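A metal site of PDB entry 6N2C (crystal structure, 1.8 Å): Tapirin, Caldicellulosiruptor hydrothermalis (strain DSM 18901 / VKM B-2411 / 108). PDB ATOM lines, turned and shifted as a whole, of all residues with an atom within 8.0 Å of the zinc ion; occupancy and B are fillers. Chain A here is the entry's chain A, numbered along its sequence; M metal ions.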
ATOM      1  N   THR A 203      18.240  27.952 -21.500  1.00  0.00           N
ATOM      2  CA  THR A 203      17.492  28.975 -22.195  1.00  0.00           C
ATOM      3  C   THR A 203      17.903  30.291 -21.548  1.00  0.00           C
ATOM      4  O   THR A 203      17.748  30.436 -20.344  1.00  0.00           O
ATOM      5  CB  THR A 203      15.983  28.749 -22.091  1.00  0.00           C
ATOM      6  OG1 THR A 203      15.633  27.408 -22.507  1.00  0.00           O
ATOM      7  CG2 THR A 203      15.209  29.742 -22.973  1.00  0.00           C
ATOM      8  N   ASN A 511       9.348  24.769  -7.073  1.00  0.00           N
ATOM      9  CA  ASN A 511      10.614  25.429  -7.423  1.00  0.00           C
ATOM     10  C   ASN A 511      10.558  26.976  -7.200  1.00  0.00           C
ATOM     11  O   ASN A 511       9.621  27.652  -7.627  1.00  0.00           O
ATOM     12  CB  ASN A 511      10.974  25.140  -8.890  1.00  0.00           C
ATOM     13  CG  ASN A 511      12.411  25.487  -9.244  1.00  0.00           C
ATOM     14  OD1 ASN A 511      13.296  24.673  -9.020  1.00  0.00           O
ATOM     15  ND2 ASN A 511      12.623  26.575  -9.908  1.00  0.00           N
ATOM     16  N   GLN A 513      12.927  30.583  -7.554  1.00  0.00           N
ATOM     17  CA  GLN A 513      13.988  31.156  -8.319  1.00  0.00           C
ATOM     18  C   GLN A 513      15.191  31.379  -7.488  1.00  0.00           C
ATOM     19  O   GLN A 513      15.102  31.658  -6.314  1.00  0.00           O
ATOM     20  CB  GLN A 513      13.545  32.426  -9.018  1.00  0.00           C
ATOM     21  CG  GLN A 513      12.253  32.354  -9.883  1.00  0.00           C
ATOM     22  CD  GLN A 513      11.634  33.648 -10.304  1.00  0.00           C
ATOM     23  OE1 GLN A 513      12.038  34.728  -9.809  1.00  0.00           O
ATOM     24  NE2 GLN A 513      10.585  33.590 -11.156  1.00  0.00           N
ATOM     25  N   ASN A 529      17.924  19.800 -10.744  1.00  0.00           N
ATOM     26  CA  ASN A 529      17.433  19.515 -12.046  1.00  0.00           C
ATOM     27  C   ASN A 529      16.660  20.633 -12.739  1.00  0.00           C
ATOM     28  O   ASN A 529      16.364  20.533 -13.917  1.00  0.00           O
ATOM     29  CB  ASN A 529      16.602  18.256 -12.008  1.00  0.00           C
ATOM     30  CG  ASN A 529      15.316  18.428 -11.214  1.00  0.00           C
ATOM     31  OD1 ASN A 529      14.906  19.518 -10.835  1.00  0.00           O
ATOM     32  ND2 ASN A 529      14.693  17.314 -10.926  1.00  0.00           N
ATOM     33  N   HIS A 530      16.324  21.710 -12.005  1.00  0.00           N
ATOM     34  CA  HIS A 530      15.595  22.805 -12.619  1.00  0.00           C
ATOM     35  C   HIS A 530      15.992  24.075 -11.877  1.00  0.00           C
ATOM     36  O   HIS A 530      15.750  24.202 -10.689  1.00  0.00           O
ATOM     37  CB  HIS A 530      14.071  22.576 -12.485  1.00  0.00           C
ATOM     38  CG  HIS A 530      13.222  23.677 -13.094  1.00  0.00           C
ATOM     39  ND1 HIS A 530      11.937  23.950 -12.671  1.00  0.00           N
ATOM     40  CD2 HIS A 530      13.493  24.571 -14.063  1.00  0.00           C
ATOM     41  CE1 HIS A 530      11.474  24.983 -13.352  1.00  0.00           C
ATOM     42  NE2 HIS A 530      12.399  25.378 -14.227  1.00  0.00           N
ATOM     43  N   LEU A 531      16.586  25.001 -12.606  1.00  0.00           N
ATOM     44  CA  LEU A 531      16.969  26.290 -12.044  1.00  0.00           C
ATOM     45  C   LEU A 531      16.489  27.444 -12.911  1.00  0.00           C
ATOM     46  O   LEU A 531      16.886  27.558 -14.100  1.00  0.00           O
ATOM     47  CB  LEU A 531      18.497  26.378 -11.893  1.00  0.00           C
ATOM     48  CG  LEU A 531      19.135  25.635 -10.742  1.00  0.00           C
ATOM     49  CD1 LEU A 531      20.644  25.448 -10.972  1.00  0.00           C
ATOM     50  CD2 LEU A 531      18.898  26.415  -9.447  1.00  0.00           C
ATOM     51  N   ASP A 532      15.711  28.355 -12.300  1.00  0.00           N
ATOM     52  CA  ASP A 532      15.261  29.577 -12.955  1.00  0.00           C
ATOM     53  C   ASP A 532      15.927  30.704 -12.220  1.00  0.00           C
ATOM     54  O   ASP A 532      15.820  30.781 -10.983  1.00  0.00           O
ATOM     55  CB  ASP A 532      13.751  29.753 -12.747  1.00  0.00           C
ATOM     56  CG  ASP A 532      12.911  28.818 -13.595  1.00  0.00           C
ATOM     57  OD1 ASP A 532      13.437  28.402 -14.627  1.00  0.00           O
ATOM     58  OD2 ASP A 532      11.797  28.618 -13.258  1.00  0.00           O
ATOM     59  N   GLY A 533      16.606  31.558 -12.955  1.00  0.00           N
ATOM     60  CA  GLY A 533      17.274  32.672 -12.343  1.00  0.00           C
ATOM     61  C   GLY A 533      18.538  33.030 -13.056  1.00  0.00           C
ATOM     62  O   GLY A 533      18.542  33.116 -14.307  1.00  0.00           O
ATOM     63  N   ASN A 549      17.643  21.578 -16.397  1.00  0.00           N
ATOM     64  CA  ASN A 549      17.129  22.614 -17.271  1.00  0.00           C
ATOM     65  C   ASN A 549      17.383  23.958 -16.486  1.00  0.00           C
ATOM     66  O   ASN A 549      16.991  24.070 -15.327  1.00  0.00           O
ATOM     67  CB  ASN A 549      15.645  22.472 -17.427  1.00  0.00           C
ATOM     68  CG  ASN A 549      15.261  21.295 -18.227  1.00  0.00           C
ATOM     69  OD1 ASN A 549      15.697  21.130 -19.401  1.00  0.00           O
ATOM     70  ND2 ASN A 549      14.438  20.402 -17.615  1.00  0.00           N
ATOM     71  N   ILE A 550      18.008  24.907 -17.190  1.00  0.00           N
ATOM     72  CA  ILE A 550      18.377  26.244 -16.713  1.00  0.00           C
ATOM     73  C   ILE A 550      17.575  27.198 -17.541  1.00  0.00           C
ATOM     74  O   ILE A 550      17.625  27.190 -18.771  1.00  0.00           O
ATOM     75  CB  ILE A 550      19.916  26.547 -16.826  1.00  0.00           C
ATOM     76  CG1 ILE A 550      20.676  25.545 -15.976  1.00  0.00           C
ATOM     77  CG2 ILE A 550      20.231  27.980 -16.318  1.00  0.00           C
ATOM     78  CD1 ILE A 550      22.121  25.466 -16.265  1.00  0.00           C
ATOM     79  N   GLU A 551      16.821  28.085 -16.881  1.00  0.00           N
ATOM     80  CA  GLU A 551      16.149  29.135 -17.629  1.00  0.00           C
ATOM     81  C   GLU A 551      16.424  30.518 -16.938  1.00  0.00           C
ATOM     82  O   GLU A 551      16.301  30.624 -15.738  1.00  0.00           O
ATOM     83  CB  GLU A 551      14.645  28.932 -17.592  1.00  0.00           C
ATOM     84  CG  GLU A 551      14.051  27.774 -18.470  1.00  0.00           C
ATOM     85  CD  GLU A 551      14.184  26.387 -17.830  1.00  0.00           C
ATOM     86  OE1 GLU A 551      13.755  26.224 -16.680  1.00  0.00           O
ATOM     87  OE2 GLU A 551      14.768  25.449 -18.454  1.00  0.00           O
ATOM     88  N   TYR A 552      16.809  31.451 -17.757  1.00  0.00           N
ATOM     89  CA  TYR A 552      17.005  32.832 -17.302  1.00  0.00           C
ATOM     90  C   TYR A 552      15.645  33.399 -16.822  1.00  0.00           C
ATOM     91  O   TYR A 552      14.608  33.342 -17.583  1.00  0.00           O
ATOM     92  CB  TYR A 552      17.489  33.670 -18.451  1.00  0.00           C
ATOM     93  CG  TYR A 552      17.432  35.195 -18.271  1.00  0.00           C
ATOM     94  CD1 TYR A 552      18.317  35.830 -17.420  1.00  0.00           C
ATOM     95  CD2 TYR A 552      16.405  35.980 -18.848  1.00  0.00           C
ATOM     96  CE1 TYR A 552      18.258  37.200 -17.261  1.00  0.00           C
ATOM     97  CE2 TYR A 552      16.360  37.358 -18.657  1.00  0.00           C
ATOM     98  CZ  TYR A 552      17.352  37.964 -17.936  1.00  0.00           C
ATOM     99  OH  TYR A 552      17.297  39.328 -17.687  1.00  0.00           O
ATOM    100  N   VAL A 553      15.712  34.054 -15.692  1.00  0.00           N
ATOM    101  CA  VAL A 553      14.675  34.955 -15.275  1.00  0.00           C
ATOM    102  C   VAL A 553      15.395  36.244 -14.819  1.00  0.00           C
ATOM    103  O   VAL A 553      16.359  36.151 -14.062  1.00  0.00           O
ATOM    104  CB  VAL A 553      13.899  34.377 -14.074  1.00  0.00           C
ATOM    105  CG1 VAL A 553      12.952  35.400 -13.364  1.00  0.00           C
ATOM    106  CG2 VAL A 553      13.145  33.122 -14.487  1.00  0.00           C
HETATM  107 ZN    ZN M   1      12.396  26.898 -15.409  1.00  0.00          ZN
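N of Glu 551 sits at hydrogen-bond distance from O of Leu 531, 2.8 Å away.
O of His 530 sits close to OD1 of Asn 511 (3.0 Å).
The backbone NH (N) of Gly 533 is in hydrogen-bond range of the backbone carbonyl oxygen (O) of Glu 551 (3.0 Å).
The zinc ion is bound by NE2 of His 530, OE1 of Glu 551 and OD1 of Asp 532.
The zinc ion has three donor atoms within binding distance.
Slightly farther from the zinc ion lies the side-chain carboxylate (OD2) of Asp 532 (2.8 Å).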
